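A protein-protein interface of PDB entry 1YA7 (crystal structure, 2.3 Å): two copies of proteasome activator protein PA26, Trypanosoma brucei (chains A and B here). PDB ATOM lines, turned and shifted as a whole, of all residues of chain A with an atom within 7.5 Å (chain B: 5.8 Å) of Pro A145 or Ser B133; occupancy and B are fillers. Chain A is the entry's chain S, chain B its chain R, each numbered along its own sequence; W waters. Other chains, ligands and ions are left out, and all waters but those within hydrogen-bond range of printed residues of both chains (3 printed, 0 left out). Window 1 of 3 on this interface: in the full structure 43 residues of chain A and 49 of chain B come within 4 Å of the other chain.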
ATOM      1  N   TYR A  80      -2.681 -11.339 -28.205  1.00  0.00           N
ATOM      2  CA  TYR A  80      -2.484 -12.146 -27.010  1.00  0.00           C
ATOM      3  C   TYR A  80      -1.810 -11.360 -25.867  1.00  0.00           C
ATOM      4  O   TYR A  80      -2.272 -11.402 -24.742  1.00  0.00           O
ATOM      5  CB  TYR A  80      -1.733 -13.433 -27.300  1.00  0.00           C
ATOM      6  CG  TYR A  80      -1.695 -14.326 -26.078  1.00  0.00           C
ATOM      7  CD1 TYR A  80      -2.885 -14.751 -25.482  1.00  0.00           C
ATOM      8  CD2 TYR A  80      -0.486 -14.739 -25.505  1.00  0.00           C
ATOM      9  CE1 TYR A  80      -2.891 -15.565 -24.374  1.00  0.00           C
ATOM     10  CE2 TYR A  80      -0.484 -15.582 -24.366  1.00  0.00           C
ATOM     11  CZ  TYR A  80      -1.706 -15.978 -23.825  1.00  0.00           C
ATOM     12  OH  TYR A  80      -1.787 -16.786 -22.713  1.00  0.00           O
ATOM     13  N   LYS A 129       2.161 -18.213 -13.002  1.00  0.00           N
ATOM     14  CA  LYS A 129       2.308 -19.348 -13.915  1.00  0.00           C
ATOM     15  C   LYS A 129       1.560 -19.160 -15.270  1.00  0.00           C
ATOM     16  O   LYS A 129       2.198 -19.147 -16.324  1.00  0.00           O
ATOM     17  CB  LYS A 129       1.919 -20.665 -13.230  1.00  0.00           C
ATOM     18  CG  LYS A 129       2.860 -21.090 -12.086  1.00  0.00           C
ATOM     19  CD  LYS A 129       2.364 -22.428 -11.504  1.00  0.00           C
ATOM     20  CE  LYS A 129       2.987 -22.726 -10.140  1.00  0.00           C
ATOM     21  NZ  LYS A 129       2.651 -24.128  -9.700  1.00  0.00           N
ATOM     22  N   THR A 130       0.235 -18.994 -15.244  1.00  0.00           N
ATOM     23  CA  THR A 130      -0.549 -18.922 -16.478  1.00  0.00           C
ATOM     24  C   THR A 130      -0.130 -17.772 -17.408  1.00  0.00           C
ATOM     25  O   THR A 130       0.120 -18.000 -18.594  1.00  0.00           O
ATOM     26  CB  THR A 130      -2.083 -18.902 -16.175  1.00  0.00           C
ATOM     27  OG1 THR A 130      -2.381 -19.925 -15.223  1.00  0.00           O
ATOM     28  CG2 THR A 130      -2.911 -19.317 -17.399  1.00  0.00           C
ATOM     29  N   ALA A 142       8.259 -23.098 -16.252  1.00  0.00           N
ATOM     30  CA  ALA A 142       7.136 -22.340 -16.831  1.00  0.00           C
ATOM     31  C   ALA A 142       6.151 -23.264 -17.598  1.00  0.00           C
ATOM     32  O   ALA A 142       6.357 -23.587 -18.786  1.00  0.00           O
ATOM     33  CB  ALA A 142       7.654 -21.204 -17.720  1.00  0.00           C
ATOM     34  N   PRO A 143       5.088 -23.675 -16.902  1.00  0.00           N
ATOM     35  CA  PRO A 143       4.109 -24.664 -17.405  1.00  0.00           C
ATOM     36  C   PRO A 143       3.141 -24.138 -18.482  1.00  0.00           C
ATOM     37  O   PRO A 143       2.421 -24.922 -19.117  1.00  0.00           O
ATOM     38  CB  PRO A 143       3.304 -25.014 -16.140  1.00  0.00           C
ATOM     39  CG  PRO A 143       3.329 -23.739 -15.350  1.00  0.00           C
ATOM     40  CD  PRO A 143       4.731 -23.201 -15.549  1.00  0.00           C
ATOM     41  N   THR A 144       3.098 -22.823 -18.658  1.00  0.00           N
ATOM     42  CA  THR A 144       2.288 -22.242 -19.711  1.00  0.00           C
ATOM     43  C   THR A 144       3.042 -22.406 -21.041  1.00  0.00           C
ATOM     44  O   THR A 144       4.273 -22.282 -21.063  1.00  0.00           O
ATOM     45  CB  THR A 144       1.944 -20.768 -19.391  1.00  0.00           C
ATOM     46  OG1 THR A 144       1.067 -20.257 -20.403  1.00  0.00           O
ATOM     47  CG2 THR A 144       3.203 -19.847 -19.470  1.00  0.00           C
ATOM     48  N   PRO A 145       2.337 -22.762 -22.125  1.00  0.00           N
ATOM     49  CA  PRO A 145       2.985 -22.882 -23.457  1.00  0.00           C
ATOM     50  C   PRO A 145       3.730 -21.619 -23.925  1.00  0.00           C
ATOM     51  O   PRO A 145       4.739 -21.735 -24.621  1.00  0.00           O
ATOM     52  CB  PRO A 145       1.831 -23.247 -24.381  1.00  0.00           C
ATOM     53  CG  PRO A 145       0.880 -23.946 -23.462  1.00  0.00           C
ATOM     54  CD  PRO A 145       0.917 -23.163 -22.172  1.00  0.00           C
ATOM     55  N   ILE A 146       3.260 -20.446 -23.503  1.00  0.00           N
ATOM     56  CA  ILE A 146       3.853 -19.147 -23.873  1.00  0.00           C
ATOM     57  C   ILE A 146       3.326 -18.108 -22.891  1.00  0.00           C
ATOM     58  O   ILE A 146       2.192 -18.225 -22.444  1.00  0.00           O
ATOM     59  CB  ILE A 146       3.486 -18.754 -25.370  1.00  0.00           C
ATOM     60  CG1 ILE A 146       4.384 -17.646 -25.899  1.00  0.00           C
ATOM     61  CG2 ILE A 146       2.061 -18.291 -25.519  1.00  0.00           C
ATOM     62  CD1 ILE A 146       5.780 -18.118 -26.248  1.00  0.00           C
ATOM     63  N   GLY A 147       4.124 -17.095 -22.563  1.00  0.00           N
ATOM     64  CA  GLY A 147       3.661 -16.054 -21.650  1.00  0.00           C
ATOM     65  C   GLY A 147       3.386 -14.662 -22.200  1.00  0.00           C
ATOM     66  O   GLY A 147       3.395 -14.438 -23.395  1.00  0.00           O
ATOM     67  N   GLU A 153       9.690 -12.969 -27.336  1.00  0.00           N
ATOM     68  CA  GLU A 153      10.147 -14.366 -27.431  1.00  0.00           C
ATOM     69  C   GLU A 153      10.189 -14.814 -28.910  1.00  0.00           C
ATOM     70  O   GLU A 153      11.137 -15.427 -29.367  1.00  0.00           O
ATOM     71  CB  GLU A 153       9.184 -15.297 -26.668  1.00  0.00           C
ATOM     72  CG  GLU A 153       9.167 -15.266 -25.130  1.00  0.00           C
ATOM     73  CD  GLU A 153       8.277 -16.395 -24.548  1.00  0.00           C
ATOM     74  OE1 GLU A 153       7.515 -16.158 -23.568  1.00  0.00           O
ATOM     75  OE2 GLU A 153       8.321 -17.547 -25.093  1.00  0.00           O
ATOM     76  N   ASP A 195       5.039 -23.040 -34.570  1.00  0.00           N
ATOM     77  CA  ASP A 195       5.015 -23.344 -33.117  1.00  0.00           C
ATOM     78  C   ASP A 195       4.570 -22.188 -32.267  1.00  0.00           C
ATOM     79  O   ASP A 195       3.861 -22.386 -31.271  1.00  0.00           O
ATOM     80  CB  ASP A 195       6.387 -23.781 -32.635  1.00  0.00           C
ATOM     81  CG  ASP A 195       6.702 -25.211 -33.007  1.00  0.00           C
ATOM     82  OD1 ASP A 195       5.844 -25.895 -33.640  1.00  0.00           O
ATOM     83  OD2 ASP A 195       7.784 -25.733 -32.686  1.00  0.00           O
ATOM     84  N   PHE A 196       4.952 -20.972 -32.643  1.00  0.00           N
ATOM     85  CA  PHE A 196       4.432 -19.819 -31.946  1.00  0.00           C
ATOM     86  C   PHE A 196       2.931 -19.622 -32.071  1.00  0.00           C
ATOM     87  O   PHE A 196       2.299 -19.183 -31.089  1.00  0.00           O
ATOM     88  CB  PHE A 196       5.242 -18.552 -32.250  1.00  0.00           C
ATOM     89  CG  PHE A 196       6.456 -18.430 -31.368  1.00  0.00           C
ATOM     90  CD1 PHE A 196       7.645 -19.071 -31.707  1.00  0.00           C
ATOM     91  CD2 PHE A 196       6.375 -17.778 -30.135  1.00  0.00           C
ATOM     92  CE1 PHE A 196       8.793 -18.995 -30.852  1.00  0.00           C
ATOM     93  CE2 PHE A 196       7.497 -17.719 -29.261  1.00  0.00           C
ATOM     94  CZ  PHE A 196       8.699 -18.319 -29.617  1.00  0.00           C
ATOM     95  N   LEU A 198       0.899 -22.143 -32.578  1.00  0.00           N
ATOM     96  CA  LEU A 198       0.436 -23.273 -31.801  1.00  0.00           C
ATOM     97  C   LEU A 198       0.461 -22.963 -30.285  1.00  0.00           C
ATOM     98  O   LEU A 198      -0.454 -23.340 -29.548  1.00  0.00           O
ATOM     99  CB  LEU A 198       1.331 -24.470 -32.076  1.00  0.00           C
ATOM    100  CG  LEU A 198       1.106 -25.642 -31.118  1.00  0.00           C
ATOM    101  CD1 LEU A 198      -0.356 -26.109 -31.218  1.00  0.00           C
ATOM    102  CD2 LEU A 198       2.080 -26.793 -31.464  1.00  0.00           C
ATOM    103  N   LYS A 199       1.538 -22.319 -29.830  1.00  0.00           N
ATOM    104  CA  LYS A 199       1.699 -21.987 -28.422  1.00  0.00           C
ATOM    105  C   LYS A 199       0.576 -21.081 -27.967  1.00  0.00           C
ATOM    106  O   LYS A 199      -0.019 -21.307 -26.929  1.00  0.00           O
ATOM    107  CB  LYS A 199       3.076 -21.337 -28.170  1.00  0.00           C
ATOM    108  CG  LYS A 199       4.200 -22.348 -28.165  1.00  0.00           C
ATOM    109  CD  LYS A 199       5.555 -21.655 -28.132  1.00  0.00           C
ATOM    110  CE  LYS A 199       6.579 -22.646 -27.567  1.00  0.00           C
ATOM    111  NZ  LYS A 199       7.940 -22.148 -27.830  1.00  0.00           N
ATOM    112  N   VAL A 200       0.265 -20.070 -28.759  1.00  0.00           N
ATOM    113  CA  VAL A 200      -0.926 -19.231 -28.506  1.00  0.00           C
ATOM    114  C   VAL A 200      -2.233 -20.015 -28.410  1.00  0.00           C
ATOM    115  O   VAL A 200      -3.053 -19.742 -27.511  1.00  0.00           O
ATOM    116  CB  VAL A 200      -1.078 -18.148 -29.568  1.00  0.00           C
ATOM    117  CG1 VAL A 200      -2.406 -17.404 -29.395  1.00  0.00           C
ATOM    118  CG2 VAL A 200       0.103 -17.186 -29.488  1.00  0.00           C
ATOM    119  N   GLU A 201      -2.440 -20.981 -29.320  1.00  0.00           N
ATOM    120  CA  GLU A 201      -3.661 -21.825 -29.271  1.00  0.00           C
ATOM    121  C   GLU A 201      -3.724 -22.563 -27.940  1.00  0.00           C
ATOM    122  O   GLU A 201      -4.763 -22.616 -27.315  1.00  0.00           O
ATOM    123  CB  GLU A 201      -3.690 -22.874 -30.367  1.00  0.00           C
ATOM    124  CG  GLU A 201      -3.616 -22.365 -31.789  1.00  0.00           C
ATOM    125  CD  GLU A 201      -3.682 -23.533 -32.778  1.00  0.00           C
ATOM    126  OE1 GLU A 201      -2.718 -23.712 -33.558  1.00  0.00           O
ATOM    127  OE2 GLU A 201      -4.695 -24.292 -32.745  1.00  0.00           O
ATOM    128  N   LEU A 202      -2.593 -23.133 -27.530  1.00  0.00           N
ATOM    129  CA  LEU A 202      -2.521 -23.879 -26.288  1.00  0.00           C
ATOM    130  C   LEU A 202      -2.646 -22.952 -25.078  1.00  0.00           C
ATOM    131  O   LEU A 202      -3.388 -23.261 -24.144  1.00  0.00           O
ATOM    132  CB  LEU A 202      -1.224 -24.686 -26.234  1.00  0.00           C
ATOM    133  CG  LEU A 202      -0.963 -25.727 -27.336  1.00  0.00           C
ATOM    134  CD1 LEU A 202       0.321 -26.461 -27.017  1.00  0.00           C
ATOM    135  CD2 LEU A 202      -2.085 -26.735 -27.481  1.00  0.00           C
ATOM    136  N   ALA A 203      -1.959 -21.805 -25.100  1.00  0.00           N
ATOM    137  CA  ALA A 203      -1.991 -20.889 -23.943  1.00  0.00           C
ATOM    138  C   ALA A 203      -3.372 -20.263 -23.712  1.00  0.00           C
ATOM    139  O   ALA A 203      -3.801 -20.142 -22.565  1.00  0.00           O
ATOM    140  CB  ALA A 203      -0.908 -19.812 -24.063  1.00  0.00           C
ATOM    141  N   THR A 204      -4.085 -19.898 -24.782  1.00  0.00           N
ATOM    142  CA  THR A 204      -5.473 -19.366 -24.648  1.00  0.00           C
ATOM    143  C   THR A 204      -6.420 -20.389 -24.057  1.00  0.00           C
ATOM    144  O   THR A 204      -7.266 -20.058 -23.202  1.00  0.00           O
ATOM    145  CB  THR A 204      -6.059 -18.861 -26.008  1.00  0.00           C
ATOM    146  OG1 THR A 204      -5.785 -19.827 -27.034  1.00  0.00           O
ATOM    147  CG2 THR A 204      -5.349 -17.570 -26.471  1.00  0.00           C
ATOM    148  N   HIS A 206      -5.540 -22.984 -22.123  1.00  0.00           N
ATOM    149  CA  HIS A 206      -5.095 -23.043 -20.745  1.00  0.00           C
ATOM    150  C   HIS A 206      -5.541 -21.818 -19.921  1.00  0.00           C
ATOM    151  O   HIS A 206      -6.063 -21.947 -18.822  1.00  0.00           O
ATOM    152  CB  HIS A 206      -3.579 -23.195 -20.740  1.00  0.00           C
ATOM    153  CG  HIS A 206      -3.017 -23.553 -19.411  1.00  0.00           C
ATOM    154  ND1 HIS A 206      -3.361 -24.716 -18.751  1.00  0.00           N
ATOM    155  CD2 HIS A 206      -2.109 -22.920 -18.624  1.00  0.00           C
ATOM    156  CE1 HIS A 206      -2.699 -24.776 -17.608  1.00  0.00           C
ATOM    157  NE2 HIS A 206      -1.936 -23.699 -17.507  1.00  0.00           N
ATOM    158  N   LEU A 207      -5.395 -20.628 -20.474  1.00  0.00           N
ATOM    159  CA  LEU A 207      -5.854 -19.439 -19.770  1.00  0.00           C
ATOM    160  C   LEU A 207      -7.398 -19.439 -19.585  1.00  0.00           C
ATOM    161  O   LEU A 207      -7.917 -19.007 -18.546  1.00  0.00           O
ATOM    162  CB  LEU A 207      -5.369 -18.192 -20.524  1.00  0.00           C
ATOM    163  CG  LEU A 207      -5.789 -16.852 -19.923  1.00  0.00           C
ATOM    164  CD1 LEU A 207      -5.263 -16.742 -18.465  1.00  0.00           C
ATOM    165  CD2 LEU A 207      -5.305 -15.663 -20.775  1.00  0.00           C
ATOM    166  N   TYR B  88      -3.792 -32.355 -25.510  1.00  0.00           N
ATOM    167  CA  TYR B  88      -3.719 -31.175 -24.641  1.00  0.00           C
ATOM    168  C   TYR B  88      -5.062 -30.473 -24.566  1.00  0.00           C
ATOM    169  O   TYR B  88      -5.578 -30.240 -23.474  1.00  0.00           O
ATOM    170  CB  TYR B  88      -2.642 -30.205 -25.124  1.00  0.00           C
ATOM    171  CG  TYR B  88      -2.402 -29.056 -24.181  1.00  0.00           C
ATOM    172  CD1 TYR B  88      -1.423 -29.144 -23.192  1.00  0.00           C
ATOM    173  CD2 TYR B  88      -3.161 -27.869 -24.274  1.00  0.00           C
ATOM    174  CE1 TYR B  88      -1.198 -28.080 -22.314  1.00  0.00           C
ATOM    175  CE2 TYR B  88      -2.943 -26.824 -23.418  1.00  0.00           C
ATOM    176  CZ  TYR B  88      -1.951 -26.933 -22.440  1.00  0.00           C
ATOM    177  OH  TYR B  88      -1.717 -25.895 -21.577  1.00  0.00           O
ATOM    178  N   GLU B 127      -0.542 -33.258 -19.080  1.00  0.00           N
ATOM    179  CA  GLU B 127      -0.307 -32.033 -19.847  1.00  0.00           C
ATOM    180  C   GLU B 127       1.125 -31.539 -19.747  1.00  0.00           C
ATOM    181  O   GLU B 127       1.735 -31.167 -20.748  1.00  0.00           O
ATOM    182  CB  GLU B 127      -1.275 -30.946 -19.388  1.00  0.00           C
ATOM    183  CG  GLU B 127      -2.729 -31.207 -19.746  1.00  0.00           C
ATOM    184  CD  GLU B 127      -3.563 -29.942 -19.665  1.00  0.00           C
ATOM    185  OE1 GLU B 127      -2.996 -28.866 -19.888  1.00  0.00           O
ATOM    186  OE2 GLU B 127      -4.775 -29.987 -19.384  1.00  0.00           O
ATOM    187  N   ILE B 128       1.659 -31.577 -18.534  1.00  0.00           N
ATOM    188  CA  ILE B 128       2.922 -30.931 -18.202  1.00  0.00           C
ATOM    189  C   ILE B 128       4.099 -31.870 -18.385  1.00  0.00           C
ATOM    190  O   ILE B 128       4.989 -31.584 -19.176  1.00  0.00           O
ATOM    191  CB  ILE B 128       2.860 -30.310 -16.761  1.00  0.00           C
ATOM    192  CG1 ILE B 128       1.806 -29.188 -16.721  1.00  0.00           C
ATOM    193  CG2 ILE B 128       4.236 -29.805 -16.283  1.00  0.00           C
ATOM    194  CD1 ILE B 128       1.938 -28.180 -17.877  1.00  0.00           C
ATOM    195  N   LEU B 131       3.270 -34.589 -21.996  1.00  0.00           N
ATOM    196  CA  LEU B 131       3.204 -33.908 -23.273  1.00  0.00           C
ATOM    197  C   LEU B 131       4.280 -32.824 -23.408  1.00  0.00           C
ATOM    198  O   LEU B 131       4.446 -32.263 -24.489  1.00  0.00           O
ATOM    199  CB  LEU B 131       1.827 -33.296 -23.505  1.00  0.00           C
ATOM    200  CG  LEU B 131       0.574 -34.140 -23.710  1.00  0.00           C
ATOM    201  CD1 LEU B 131      -0.610 -33.203 -23.885  1.00  0.00           C
ATOM    202  CD2 LEU B 131       0.668 -35.093 -24.896  1.00  0.00           C
ATOM    203  N   GLY B 132       4.999 -32.528 -22.320  1.00  0.00           N
ATOM    204  CA  GLY B 132       5.971 -31.432 -22.322  1.00  0.00           C
ATOM    205  C   GLY B 132       5.462 -30.188 -23.031  1.00  0.00           C
ATOM    206  O   GLY B 132       6.071 -29.716 -23.973  1.00  0.00           O
ATOM    207  N   SER B 133       4.335 -29.663 -22.571  1.00  0.00           N
ATOM    208  CA  SER B 133       3.697 -28.503 -23.196  1.00  0.00           C
ATOM    209  C   SER B 133       4.196 -27.134 -22.720  1.00  0.00           C
ATOM    210  O   SER B 133       3.993 -26.144 -23.417  1.00  0.00           O
ATOM    211  CB  SER B 133       2.188 -28.559 -23.007  1.00  0.00           C
ATOM    212  OG  SER B 133       1.880 -28.495 -21.632  1.00  0.00           O
ATOM    213  N   GLY B 134       4.824 -27.077 -21.541  1.00  0.00           N
ATOM    214  CA  GLY B 134       5.324 -25.813 -20.983  1.00  0.00           C
ATOM    215  C   GLY B 134       6.567 -25.315 -21.698  1.00  0.00           C
ATOM    216  O   GLY B 134       7.264 -26.106 -22.337  1.00  0.00           O
ATOM    217  N   GLU B 135       6.840 -24.012 -21.593  1.00  0.00           N
ATOM    218  CA  GLU B 135       8.084 -23.405 -22.097  1.00  0.00           C
ATOM    219  C   GLU B 135       9.345 -23.930 -21.391  1.00  0.00           C
ATOM    220  O   GLU B 135      10.423 -23.985 -21.987  1.00  0.00           O
ATOM    221  CB  GLU B 135       8.080 -21.898 -21.878  1.00  0.00           C
ATOM    222  CG  GLU B 135       7.086 -21.087 -22.671  1.00  0.00           C
ATOM    223  CD  GLU B 135       6.894 -19.715 -22.043  1.00  0.00           C
ATOM    224  OE1 GLU B 135       6.222 -19.623 -20.980  1.00  0.00           O
ATOM    225  OE2 GLU B 135       7.422 -18.733 -22.605  1.00  0.00           O
ATOM    226  N   MET B 148       6.007 -31.724 -26.905  1.00  0.00           N
ATOM    227  CA  MET B 148       5.148 -31.058 -27.913  1.00  0.00           C
ATOM    228  C   MET B 148       5.889 -30.441 -29.115  1.00  0.00           C
ATOM    229  O   MET B 148       5.389 -30.472 -30.248  1.00  0.00           O
ATOM    230  CB  MET B 148       4.312 -29.956 -27.208  1.00  0.00           C
ATOM    231  CG  MET B 148       3.376 -29.125 -28.097  1.00  0.00           C
ATOM    232  SD  MET B 148       1.732 -29.862 -28.296  1.00  0.00           S
ATOM    233  CE  MET B 148       1.305 -30.072 -26.570  1.00  0.00           C
ATOM    234  N   TYR B 149       7.055 -29.859 -28.858  1.00  0.00           N
ATOM    235  CA  TYR B 149       7.824 -29.144 -29.875  1.00  0.00           C
ATOM    236  C   TYR B 149       9.002 -30.002 -30.379  1.00  0.00           C
ATOM    237  O   TYR B 149      10.139 -29.532 -30.544  1.00  0.00           O
ATOM    238  CB  TYR B 149       8.246 -27.772 -29.304  1.00  0.00           C
ATOM    239  CG  TYR B 149       7.108 -27.169 -28.497  1.00  0.00           C
ATOM    240  CD1 TYR B 149       7.128 -27.196 -27.085  1.00  0.00           C
ATOM    241  CD2 TYR B 149       5.968 -26.649 -29.136  1.00  0.00           C
ATOM    242  CE1 TYR B 149       6.056 -26.683 -26.342  1.00  0.00           C
ATOM    243  CE2 TYR B 149       4.903 -26.128 -28.407  1.00  0.00           C
ATOM    244  CZ  TYR B 149       4.953 -26.142 -27.018  1.00  0.00           C
ATOM    245  OH  TYR B 149       3.903 -25.626 -26.294  1.00  0.00           O
HETATM  246  O   HOH W   1       0.565 -26.083 -20.177  1.00  0.00           O
HETATM  247  O   HOH W   2       8.056 -28.241 -32.833  1.00  0.00           O
HETATM  248  O   HOH W   3      -1.056 -27.315 -18.369  1.00  0.00           O
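Water W1 lies within hydrogen-bond range of O of Pro A143 (2.4 Å), OH of Tyr B88 (2.7 Å) and OG of Ser B133 (3.1 Å). Water W2 lies within hydrogen-bond range of OD2 of Asp A195 (2.5 Å) and O of Tyr B149 (3.4 Å). Water W3 bridges the side-chain carboxylate (OE1) of Glu B127 (2.9 Å) and a ring nitrogen (ND1) of His A206 (3.5 Å).
The side-chain hydroxyl (OH) of Tyr B88 lies close to a ring nitrogen (ND1) of His A206. The backbone carbonyl oxygen (O) of Ala A142 sits at hydrogen-bond distance from the backbone NH (N) of Glu B135 (2.9 Å). The backbone NH (N) of Glu B135 lies within hydrogen-bond range of the backbone carbonyl oxygen (O) of Thr A144 (3.1 Å). The side-chain carboxylate (OE1) of Glu A153 lies close to the side-chain carboxylate (OE2) of Glu B135, 2.8 Å away.
Of chain A, only Pro A145 (3.4 Å) comes within 4 Å of Ser B133. Of the printed residues of chain A, Ile B128 touches Pro A143 (3.5 Å). Printed residues of chain B within 4 Å of Glu A153: Glu B135. Printed residues of chain A within 4 Å of Met B148: Leu A202 (3.8 Å). Ala A203 touches none of the printed residues of chain B. The nearest printed residue of chain A that does not touch Tyr B149 is Leu A198 (4.2 Å).
The side-chain hydroxyl of Ser B133 is in hydrogen-bond range of the backbone carbonyl oxygen of Glu B127, 2.8 Å away. The backbone carbonyl oxygen of Leu B131 is in hydrogen-bond range of the backbone NH of Met B148 (2.9 Å). The backbone carbonyl oxygen of Ser B133 sits at hydrogen-bond distance from the side-chain hydroxyl of Tyr B149, 2.9 Å away. The backbone carbonyl oxygen (O) of Thr A130 sits at hydrogen-bond distance from the side-chain hydroxyl (OG1) of Thr A144 (3.0 Å). OG1 of Thr A144 lies within hydrogen-bond range of O of Ile A146 (3.1 Å).
Among the printed residues, merely in contact across the chains: Ala A142 with Gly B134 (3.3 Å), Pro A143 with Ile B128 (3.5 Å), Pro A143 with Gly B134 (3.6 Å), Thr A144 with Gly B134 (3.7 Å), Pro A145 with Tyr B88 (3.8 Å), Pro A145 with Ser B133 (3.4 Å), Pro A145 with Glu B135 (3.1 Å), Pro A145 with Tyr B149 (3.7 Å), Ile A146 with Glu B135 (3.6 Å), Gly A147 with Glu B135 (3.6 Å), Asp A195 with Tyr B149 (3.98 Å), Lys A199 with Tyr B149 (3.8 Å), Leu A202 with Tyr B88 (3.6 Å), Leu A202 with Met B148 (3.8 Å) and Leu A202 with Tyr B149 (3.7 Å).
Of the 21 printed residues of chain A, 11 touch a printed residue of chain B. Hydrophobic or aromatic side chains of chain A that line the printed part of chain B: Ala A142, Pro A143, Pro A145, Leu A202 and His A206. Hydrophobic or aromatic side chains of chain B within 4 Å of the printed part of chain A: Tyr B88, Ile B128, Met B148 and Tyr B149. Among the printed residues, no Asp or Glu carboxylate lies within 4 Å of a Lys or Arg side-chain nitrogen of the other chain.
No position is printed for both chains. Of the 19 pairs that touch across the chains among the printed residues, none has its exchanged pair printed and touching as well.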
